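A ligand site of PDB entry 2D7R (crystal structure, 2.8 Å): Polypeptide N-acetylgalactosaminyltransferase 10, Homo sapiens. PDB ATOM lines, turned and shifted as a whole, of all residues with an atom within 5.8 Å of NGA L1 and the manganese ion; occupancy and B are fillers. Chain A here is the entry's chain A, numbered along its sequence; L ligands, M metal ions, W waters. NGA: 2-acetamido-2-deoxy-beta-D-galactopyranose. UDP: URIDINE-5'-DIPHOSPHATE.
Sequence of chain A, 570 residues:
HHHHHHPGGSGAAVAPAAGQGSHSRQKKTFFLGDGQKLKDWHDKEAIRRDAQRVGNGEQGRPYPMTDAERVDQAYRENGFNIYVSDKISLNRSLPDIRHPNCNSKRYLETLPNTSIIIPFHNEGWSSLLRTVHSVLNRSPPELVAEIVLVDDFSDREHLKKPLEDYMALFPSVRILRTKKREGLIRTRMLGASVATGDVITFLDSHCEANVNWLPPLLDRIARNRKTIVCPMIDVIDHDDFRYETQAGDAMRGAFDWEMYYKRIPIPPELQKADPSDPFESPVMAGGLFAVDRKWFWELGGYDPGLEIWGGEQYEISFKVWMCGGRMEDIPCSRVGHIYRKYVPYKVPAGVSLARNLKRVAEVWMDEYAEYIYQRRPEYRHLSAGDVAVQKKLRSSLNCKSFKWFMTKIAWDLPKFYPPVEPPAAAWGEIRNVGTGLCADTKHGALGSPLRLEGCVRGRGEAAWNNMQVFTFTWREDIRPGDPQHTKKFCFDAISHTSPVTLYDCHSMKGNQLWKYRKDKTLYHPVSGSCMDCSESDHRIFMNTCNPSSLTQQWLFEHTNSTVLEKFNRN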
ATOM      1  N   LEU A 184      -8.203 -16.127 -14.726  1.00  0.00           N
ATOM      2  CA  LEU A 184      -8.142 -17.531 -15.100  1.00  0.00           C
ATOM      3  C   LEU A 184      -6.986 -17.900 -16.032  1.00  0.00           C
ATOM      4  O   LEU A 184      -6.329 -18.921 -15.831  1.00  0.00           O
ATOM      5  CB  LEU A 184      -9.496 -17.986 -15.660  1.00  0.00           C
ATOM      6  CG  LEU A 184     -10.060 -17.576 -17.025  1.00  0.00           C
ATOM      7  CD1 LEU A 184      -9.505 -18.458 -18.152  1.00  0.00           C
ATOM      8  CD2 LEU A 184     -11.561 -17.683 -16.976  1.00  0.00           C
ATOM      9  N   ILE A 185      -6.704 -17.069 -17.028  1.00  0.00           N
ATOM     10  CA  ILE A 185      -5.623 -17.403 -17.932  1.00  0.00           C
ATOM     11  C   ILE A 185      -4.285 -17.549 -17.213  1.00  0.00           C
ATOM     12  O   ILE A 185      -3.657 -18.609 -17.243  1.00  0.00           O
ATOM     13  CB  ILE A 185      -5.446 -16.357 -19.051  1.00  0.00           C
ATOM     14  CG1 ILE A 185      -6.707 -16.228 -19.910  1.00  0.00           C
ATOM     15  CG2 ILE A 185      -4.321 -16.793 -19.954  1.00  0.00           C
ATOM     16  CD1 ILE A 185      -7.878 -15.593 -19.242  1.00  0.00           C
ATOM     17  N   ARG A 188      -4.094 -20.393 -14.759  1.00  0.00           N
ATOM     18  CA  ARG A 188      -3.882 -21.686 -15.365  1.00  0.00           C
ATOM     19  C   ARG A 188      -2.449 -21.834 -15.828  1.00  0.00           C
ATOM     20  O   ARG A 188      -1.937 -22.954 -15.931  1.00  0.00           O
ATOM     21  CB  ARG A 188      -4.851 -21.913 -16.529  1.00  0.00           C
ATOM     22  CG  ARG A 188      -6.275 -22.050 -16.059  1.00  0.00           C
ATOM     23  CD  ARG A 188      -7.076 -22.979 -16.927  1.00  0.00           C
ATOM     24  NE  ARG A 188      -7.272 -22.428 -18.250  1.00  0.00           N
ATOM     25  CZ  ARG A 188      -8.471 -22.221 -18.795  1.00  0.00           C
ATOM     26  NH1 ARG A 188      -9.580 -22.522 -18.125  1.00  0.00           N
ATOM     27  NH2 ARG A 188      -8.548 -21.708 -20.023  1.00  0.00           N
ATOM     28  N   ASP A 204     -12.472 -27.023 -14.543  1.00  0.00           N
ATOM     29  CA  ASP A 204     -12.947 -25.866 -13.788  1.00  0.00           C
ATOM     30  C   ASP A 204     -13.173 -26.350 -12.380  1.00  0.00           C
ATOM     31  O   ASP A 204     -13.198 -27.554 -12.146  1.00  0.00           O
ATOM     32  CB  ASP A 204     -14.253 -25.333 -14.363  1.00  0.00           C
ATOM     33  CG  ASP A 204     -14.047 -24.149 -15.313  1.00  0.00           C
ATOM     34  OD1 ASP A 204     -12.882 -23.806 -15.630  1.00  0.00           O
ATOM     35  OD2 ASP A 204     -15.066 -23.564 -15.743  1.00  0.00           O
ATOM     36  N   HIS A 206     -15.744 -26.570 -10.636  1.00  0.00           N
ATOM     37  CA  HIS A 206     -17.126 -27.030 -10.388  1.00  0.00           C
ATOM     38  C   HIS A 206     -17.526 -28.004 -11.475  1.00  0.00           C
ATOM     39  O   HIS A 206     -18.462 -27.753 -12.239  1.00  0.00           O
ATOM     40  CB  HIS A 206     -18.094 -25.836 -10.371  1.00  0.00           C
ATOM     41  CG  HIS A 206     -17.693 -24.722 -11.283  1.00  0.00           C
ATOM     42  ND1 HIS A 206     -17.327 -23.479 -10.816  1.00  0.00           N
ATOM     43  CD2 HIS A 206     -17.533 -24.681 -12.621  1.00  0.00           C
ATOM     44  CE1 HIS A 206     -16.951 -22.718 -11.834  1.00  0.00           C
ATOM     45  NE2 HIS A 206     -17.067 -23.429 -12.944  1.00  0.00           N
ATOM     46  N   ILE A 233     -18.555 -31.960 -22.659  1.00  0.00           N
ATOM     47  CA  ILE A 233     -18.868 -31.229 -21.446  1.00  0.00           C
ATOM     48  C   ILE A 233     -20.371 -31.256 -21.136  1.00  0.00           C
ATOM     49  O   ILE A 233     -21.191 -30.628 -21.808  1.00  0.00           O
ATOM     50  CB  ILE A 233     -18.373 -29.789 -21.533  1.00  0.00           C
ATOM     51  CG1 ILE A 233     -16.873 -29.794 -21.847  1.00  0.00           C
ATOM     52  CG2 ILE A 233     -18.637 -29.067 -20.227  1.00  0.00           C
ATOM     53  CD1 ILE A 233     -16.318 -28.422 -22.220  1.00  0.00           C
ATOM     54  N   TYR A 261     -18.831 -17.883 -28.166  1.00  0.00           N
ATOM     55  CA  TYR A 261     -18.632 -19.281 -28.512  1.00  0.00           C
ATOM     56  C   TYR A 261     -19.939 -19.941 -28.915  1.00  0.00           C
ATOM     57  O   TYR A 261     -20.997 -19.699 -28.286  1.00  0.00           O
ATOM     58  CB  TYR A 261     -17.977 -20.029 -27.352  1.00  0.00           C
ATOM     59  CG  TYR A 261     -18.044 -21.525 -27.491  1.00  0.00           C
ATOM     60  CD1 TYR A 261     -19.056 -22.257 -26.863  1.00  0.00           C
ATOM     61  CD2 TYR A 261     -17.143 -22.217 -28.303  1.00  0.00           C
ATOM     62  CE1 TYR A 261     -19.162 -23.616 -27.028  1.00  0.00           C
ATOM     63  CE2 TYR A 261     -17.248 -23.575 -28.483  1.00  0.00           C
ATOM     64  CZ  TYR A 261     -18.251 -24.272 -27.845  1.00  0.00           C
ATOM     65  OH  TYR A 261     -18.359 -25.620 -28.038  1.00  0.00           O
ATOM     66  N   ALA A 285     -14.261 -25.488 -25.996  1.00  0.00           N
ATOM     67  CA  ALA A 285     -15.121 -24.767 -25.066  1.00  0.00           C
ATOM     68  C   ALA A 285     -14.302 -23.855 -24.156  1.00  0.00           C
ATOM     69  O   ALA A 285     -14.684 -22.695 -23.958  1.00  0.00           O
ATOM     70  CB  ALA A 285     -15.909 -25.750 -24.234  1.00  0.00           C
ATOM     71  N   GLY A 286     -13.206 -24.366 -23.597  1.00  0.00           N
ATOM     72  CA  GLY A 286     -12.387 -23.525 -22.749  1.00  0.00           C
ATOM     73  C   GLY A 286     -11.669 -24.063 -21.521  1.00  0.00           C
ATOM     74  O   GLY A 286     -10.455 -23.911 -21.381  1.00  0.00           O
ATOM     75  N   GLY A 287     -12.405 -24.681 -20.608  1.00  0.00           N
ATOM     76  CA  GLY A 287     -11.774 -25.164 -19.387  1.00  0.00           C
ATOM     77  C   GLY A 287     -11.550 -26.647 -19.241  1.00  0.00           C
ATOM     78  O   GLY A 287     -10.793 -27.074 -18.379  1.00  0.00           O
ATOM     79  N   LEU A 288     -12.184 -27.443 -20.070  1.00  0.00           N
ATOM     80  CA  LEU A 288     -12.018 -28.879 -19.980  1.00  0.00           C
ATOM     81  C   LEU A 288     -11.226 -29.374 -21.187  1.00  0.00           C
ATOM     82  O   LEU A 288     -11.768 -29.483 -22.286  1.00  0.00           O
ATOM     83  CB  LEU A 288     -13.392 -29.567 -19.962  1.00  0.00           C
ATOM     84  CG  LEU A 288     -14.311 -29.438 -18.746  1.00  0.00           C
ATOM     85  CD1 LEU A 288     -13.780 -30.313 -17.637  1.00  0.00           C
ATOM     86  CD2 LEU A 288     -14.428 -27.994 -18.308  1.00  0.00           C
ATOM     87  N   ILE A 308      -9.013 -11.300 -17.037  1.00  0.00           N
ATOM     88  CA  ILE A 308      -9.702 -12.178 -16.100  1.00  0.00           C
ATOM     89  C   ILE A 308     -10.469 -13.346 -16.687  1.00  0.00           C
ATOM     90  O   ILE A 308     -10.415 -14.455 -16.158  1.00  0.00           O
ATOM     91  CB  ILE A 308     -10.695 -11.377 -15.184  1.00  0.00           C
ATOM     92  CG1 ILE A 308      -9.924 -10.463 -14.234  1.00  0.00           C
ATOM     93  CG2 ILE A 308     -11.536 -12.336 -14.353  1.00  0.00           C
ATOM     94  CD1 ILE A 308      -9.675  -9.085 -14.777  1.00  0.00           C
ATOM     95  N   TRP A 309     -11.138 -13.117 -17.801  1.00  0.00           N
ATOM     96  CA  TRP A 309     -11.968 -14.146 -18.408  1.00  0.00           C
ATOM     97  C   TRP A 309     -12.071 -13.944 -19.924  1.00  0.00           C
ATOM     98  O   TRP A 309     -11.846 -12.843 -20.433  1.00  0.00           O
ATOM     99  CB  TRP A 309     -13.364 -14.059 -17.764  1.00  0.00           C
ATOM    100  CG  TRP A 309     -14.359 -15.049 -18.256  1.00  0.00           C
ATOM    101  CD1 TRP A 309     -14.659 -16.265 -17.709  1.00  0.00           C
ATOM    102  CD2 TRP A 309     -15.158 -14.926 -19.434  1.00  0.00           C
ATOM    103  NE1 TRP A 309     -15.600 -16.909 -18.477  1.00  0.00           N
ATOM    104  CE2 TRP A 309     -15.925 -16.112 -19.539  1.00  0.00           C
ATOM    105  CE3 TRP A 309     -15.308 -13.943 -20.410  1.00  0.00           C
ATOM    106  CZ2 TRP A 309     -16.833 -16.324 -20.585  1.00  0.00           C
ATOM    107  CZ3 TRP A 309     -16.216 -14.155 -21.455  1.00  0.00           C
ATOM    108  CH2 TRP A 309     -16.954 -15.343 -21.531  1.00  0.00           C
ATOM    109  N   GLY A 310     -12.388 -15.017 -20.645  1.00  0.00           N
ATOM    110  CA  GLY A 310     -12.554 -14.948 -22.089  1.00  0.00           C
ATOM    111  C   GLY A 310     -11.357 -14.698 -22.994  1.00  0.00           C
ATOM    112  O   GLY A 310     -10.482 -13.879 -22.691  1.00  0.00           O
ATOM    113  N   GLY A 311     -11.326 -15.418 -24.119  1.00  0.00           N
ATOM    114  CA  GLY A 311     -10.266 -15.235 -25.078  1.00  0.00           C
ATOM    115  C   GLY A 311      -9.265 -16.366 -25.244  1.00  0.00           C
ATOM    116  O   GLY A 311      -8.927 -16.720 -26.370  1.00  0.00           O
ATOM    117  N   GLU A 312      -8.775 -16.915 -24.141  1.00  0.00           N
ATOM    118  CA  GLU A 312      -7.807 -17.986 -24.241  1.00  0.00           C
ATOM    119  C   GLU A 312      -8.282 -19.220 -25.004  1.00  0.00           C
ATOM    120  O   GLU A 312      -7.448 -20.010 -25.458  1.00  0.00           O
ATOM    121  CB  GLU A 312      -7.296 -18.437 -22.875  1.00  0.00           C
ATOM    122  CG  GLU A 312      -8.165 -18.150 -21.672  1.00  0.00           C
ATOM    123  CD  GLU A 312      -9.545 -18.761 -21.734  1.00  0.00           C
ATOM    124  OE1 GLU A 312     -10.418 -18.144 -22.360  1.00  0.00           O
ATOM    125  OE2 GLU A 312      -9.743 -19.846 -21.159  1.00  0.00           O
ATOM    126  N   GLN A 313      -9.590 -19.405 -25.150  1.00  0.00           N
ATOM    127  CA  GLN A 313     -10.061 -20.599 -25.846  1.00  0.00           C
ATOM    128  C   GLN A 313      -9.867 -20.429 -27.350  1.00  0.00           C
ATOM    129  O   GLN A 313      -9.605 -21.399 -28.065  1.00  0.00           O
ATOM    130  CB  GLN A 313     -11.528 -20.924 -25.506  1.00  0.00           C
ATOM    131  CG  GLN A 313     -12.571 -20.157 -26.278  1.00  0.00           C
ATOM    132  CD  GLN A 313     -12.928 -18.844 -25.634  1.00  0.00           C
ATOM    133  OE1 GLN A 313     -12.063 -18.053 -25.277  1.00  0.00           O
ATOM    134  NE2 GLN A 313     -14.231 -18.599 -25.477  1.00  0.00           N
ATOM    135  N   HIS A 337     -20.159 -30.007 -15.777  1.00  0.00           N
ATOM    136  CA  HIS A 337     -19.729 -28.657 -15.469  1.00  0.00           C
ATOM    137  C   HIS A 337     -20.939 -27.825 -15.122  1.00  0.00           C
ATOM    138  O   HIS A 337     -21.987 -27.963 -15.750  1.00  0.00           O
ATOM    139  CB  HIS A 337     -19.010 -28.039 -16.673  1.00  0.00           C
ATOM    140  CG  HIS A 337     -18.704 -26.586 -16.513  1.00  0.00           C
ATOM    141  ND1 HIS A 337     -19.535 -25.591 -16.973  1.00  0.00           N
ATOM    142  CD2 HIS A 337     -17.692 -25.951 -15.856  1.00  0.00           C
ATOM    143  CE1 HIS A 337     -19.054 -24.418 -16.613  1.00  0.00           C
ATOM    144  NE2 HIS A 337     -17.938 -24.609 -15.936  1.00  0.00           N
ATOM    145  N   ILE A 338     -20.801 -26.961 -14.134  1.00  0.00           N
ATOM    146  CA  ILE A 338     -21.914 -26.121 -13.696  1.00  0.00           C
ATOM    147  C   ILE A 338     -21.842 -24.788 -14.372  1.00  0.00           C
ATOM    148  O   ILE A 338     -21.014 -23.979 -14.002  1.00  0.00           O
ATOM    149  CB  ILE A 338     -21.883 -25.806 -12.180  1.00  0.00           C
ATOM    150  CG1 ILE A 338     -21.749 -27.073 -11.361  1.00  0.00           C
ATOM    151  CG2 ILE A 338     -23.135 -25.078 -11.772  1.00  0.00           C
ATOM    152  CD1 ILE A 338     -21.636 -26.812  -9.860  1.00  0.00           C
ATOM    153  N   TYR A 339     -22.718 -24.557 -15.340  1.00  0.00           N
ATOM    154  CA  TYR A 339     -22.759 -23.265 -16.017  1.00  0.00           C
ATOM    155  C   TYR A 339     -23.504 -22.266 -15.117  1.00  0.00           C
ATOM    156  O   TYR A 339     -24.670 -22.461 -14.796  1.00  0.00           O
ATOM    157  CB  TYR A 339     -23.469 -23.376 -17.373  1.00  0.00           C
ATOM    158  CG  TYR A 339     -22.745 -24.205 -18.389  1.00  0.00           C
ATOM    159  CD1 TYR A 339     -22.798 -25.589 -18.340  1.00  0.00           C
ATOM    160  CD2 TYR A 339     -21.976 -23.603 -19.379  1.00  0.00           C
ATOM    161  CE1 TYR A 339     -22.095 -26.357 -19.260  1.00  0.00           C
ATOM    162  CE2 TYR A 339     -21.260 -24.366 -20.298  1.00  0.00           C
ATOM    163  CZ  TYR A 339     -21.320 -25.733 -20.234  1.00  0.00           C
ATOM    164  OH  TYR A 339     -20.606 -26.498 -21.125  1.00  0.00           O
ATOM    165  N   ARG A 340     -22.825 -21.193 -14.727  1.00  0.00           N
ATOM    166  CA  ARG A 340     -23.419 -20.192 -13.848  1.00  0.00           C
ATOM    167  C   ARG A 340     -24.655 -19.519 -14.408  1.00  0.00           C
ATOM    168  O   ARG A 340     -24.799 -19.392 -15.619  1.00  0.00           O
ATOM    169  CB  ARG A 340     -22.402 -19.100 -13.518  1.00  0.00           C
ATOM    170  CG  ARG A 340     -21.145 -19.603 -12.844  1.00  0.00           C
ATOM    171  CD  ARG A 340     -20.122 -18.514 -12.784  1.00  0.00           C
ATOM    172  NE  ARG A 340     -18.812 -19.079 -12.524  1.00  0.00           N
ATOM    173  CZ  ARG A 340     -18.294 -19.262 -11.321  1.00  0.00           C
ATOM    174  NH1 ARG A 340     -18.976 -18.922 -10.248  1.00  0.00           N
ATOM    175  NH2 ARG A 340     -17.083 -19.790 -11.212  1.00  0.00           N
HETATM  176  C1  NGA L   1     -15.655 -20.897 -21.218  1.00  0.00           C
HETATM  177  C2  NGA L   1     -14.982 -21.923 -20.299  1.00  0.00           C
HETATM  178  C3  NGA L   1     -14.294 -21.179 -19.145  1.00  0.00           C
HETATM  179  C4  NGA L   1     -13.289 -20.166 -19.703  1.00  0.00           C
HETATM  180  C5  NGA L   1     -14.022 -19.234 -20.681  1.00  0.00           C
HETATM  181  C6  NGA L   1     -13.010 -18.288 -21.321  1.00  0.00           C
HETATM  182  C7  NGA L   1     -16.038 -24.143 -20.149  1.00  0.00           C
HETATM  183  C8  NGA L   1     -17.153 -24.936 -19.474  1.00  0.00           C
HETATM  184  N2  NGA L   1     -15.979 -22.866 -19.779  1.00  0.00           N
HETATM  185  O1  NGA L   1     -16.282 -21.569 -22.321  1.00  0.00           O
HETATM  186  O3  NGA L   1     -13.604 -22.109 -18.303  1.00  0.00           O
HETATM  187  O4  NGA L   1     -12.228 -20.852 -20.372  1.00  0.00           O
HETATM  188  O5  NGA L   1     -14.662 -19.988 -21.727  1.00  0.00           O
HETATM  189  O6  NGA L   1     -12.379 -17.504 -20.302  1.00  0.00           O
HETATM  190  O7  NGA L   1     -15.275 -24.683 -20.949  1.00  0.00           O
HETATM  191  N1  UDP L   2     -11.338 -18.285 -12.106  1.00  0.00           N
HETATM  192  C2  UDP L   2     -10.099 -17.844 -11.659  1.00  0.00           C
HETATM  193  N3  UDP L   2      -9.825 -16.499 -11.657  1.00  0.00           N
HETATM  194  C4  UDP L   2     -10.751 -15.584 -12.085  1.00  0.00           C
HETATM  195  C5  UDP L   2     -12.007 -16.019 -12.547  1.00  0.00           C
HETATM  196  C6  UDP L   2     -12.250 -17.390 -12.634  1.00  0.00           C
HETATM  197  O2  UDP L   2      -9.242 -18.623 -11.259  1.00  0.00           O
HETATM  198  O4  UDP L   2     -10.468 -14.397 -12.067  1.00  0.00           O
HETATM  199  C1' UDP L   2     -11.588 -19.737 -12.114  1.00  0.00           C
HETATM  200  C2' UDP L   2     -12.975 -20.177 -11.695  1.00  0.00           C
HETATM  201  O2' UDP L   2     -13.027 -20.427 -10.304  1.00  0.00           O
HETATM  202  C3' UDP L   2     -13.193 -21.419 -12.538  1.00  0.00           C
HETATM  203  C4' UDP L   2     -12.367 -21.174 -13.794  1.00  0.00           C
HETATM  204  O4' UDP L   2     -11.438 -20.157 -13.453  1.00  0.00           O
HETATM  205  O3' UDP L   2     -12.656 -22.572 -11.912  1.00  0.00           O
HETATM  206  C5' UDP L   2     -13.174 -20.743 -15.027  1.00  0.00           C
HETATM  207  O5' UDP L   2     -13.889 -19.546 -14.785  1.00  0.00           O
HETATM  208  PA  UDP L   2     -15.505 -19.555 -14.755  1.00  0.00           P
HETATM  209  O1A UDP L   2     -16.033 -20.839 -14.253  1.00  0.00           O
HETATM  210  O2A UDP L   2     -15.969 -18.396 -13.957  1.00  0.00           O
HETATM  211  O3A UDP L   2     -15.883 -19.418 -16.303  1.00  0.00           O
HETATM  212  PB  UDP L   2     -17.189 -20.073 -16.961  1.00  0.00           P
HETATM  213  O1B UDP L   2     -17.233 -19.497 -18.325  1.00  0.00           O
HETATM  214  O2B UDP L   2     -18.410 -19.717 -16.210  1.00  0.00           O
HETATM  215  O3B UDP L   2     -17.124 -21.560 -16.986  1.00  0.00           O
HETATM  216 MN    MN M   1     -16.935 -22.730 -15.135  1.00  0.00          MN
HETATM  217  O   HOH W   1     -18.807 -21.986 -14.464  1.00  0.00           O
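Water W1 lies within hydrogen-bond range of O2B of UDP L2 (2.9 Å), O of Ile 338 (3.0 Å) and NE of Arg 340 (3.5 Å).
The backbone carbonyl oxygen (O) of Gly 286 lies within hydrogen-bond range of the guanidinium group (NH2) of Arg 188, at 3.2 Å. The backbone carbonyl oxygen of His 206 sits at hydrogen-bond distance from the backbone NH of Ile 338, 3.1 Å away. The side-chain carboxylate (OE2) of Glu 312 is in salt-bridge range of the guanidinium group (NH2) of Arg 188 (2.5 Å). O of Ile 308 lies within hydrogen-bond range of N of Leu 184, 3.1 Å away. The side-chain carboxylate (OE1) of Glu 312 lies close to the side-chain amide oxygen (OE1) of Gln 313 (3.4 Å).
O3B of UDP L2 sits close to N2 of NGA L1, at 3.3 Å.
The indole nitrogen (NE1) of Trp 309 is in hydrogen-bond range of an oxygen (O1B) of UDP L2 (3.1 Å). An oxygen (O7) of NGA L1 lies within hydrogen-bond range of the backbone NH of Gly 286, at 3.4 Å. NE of Arg 340 is in salt-bridge range of O2A of UDP L2 (3.3 Å). The backbone carbonyl oxygen of Ala 285 sits at hydrogen-bond distance from an oxygen (O1) of NGA L1. The backbone NH (N) of Gly 287 sits at hydrogen-bond distance from an oxygen (O7) of NGA L1 (2.9 Å). O4 of NGA L1 is in hydrogen-bond range of OE2 of Glu 312 (2.8 Å). The side-chain carboxylate (OD1) of Asp 204 sits at hydrogen-bond distance from an oxygen (O3) of NGA L1. The backbone NH of Gly 310 lies within hydrogen-bond range of an oxygen (O6) of NGA L1, 2.5 Å away.
Leu 184 touches NGA L1 (CD2 to O6, 3.4 Å). Arg 188 touches NGA L1. Trp 309 touches NGA L1. Hydrophobic or aromatic side chains that line NGA L1: Leu 184, Ala 285, Trp 309 and His 337. Ten residues have an atom within 4 Å of NGA L1: Leu 184, Arg 188, Asp 204, Ala 285, Gly 286, Gly 287, Trp 309, Gly 310, Glu 312 and His 337.
Water W1 is bound to the manganese ion (2.1 Å). The side-chain carboxylate (OD2) of Asp 204 binds the manganese ion, 2.1 Å away. O3B of UDP L2 binds the manganese ion (2.2 Å). O1A of UDP L2 is bound to the manganese ion, at 2.3 Å. A ring nitrogen (NE2) of His 337 is bound to the manganese ion (2.3 Å). NE2 of His 206 is bound to the manganese ion (2.3 Å).
Of the 21 residues printed, 3 come within 4 Å of the manganese ion.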
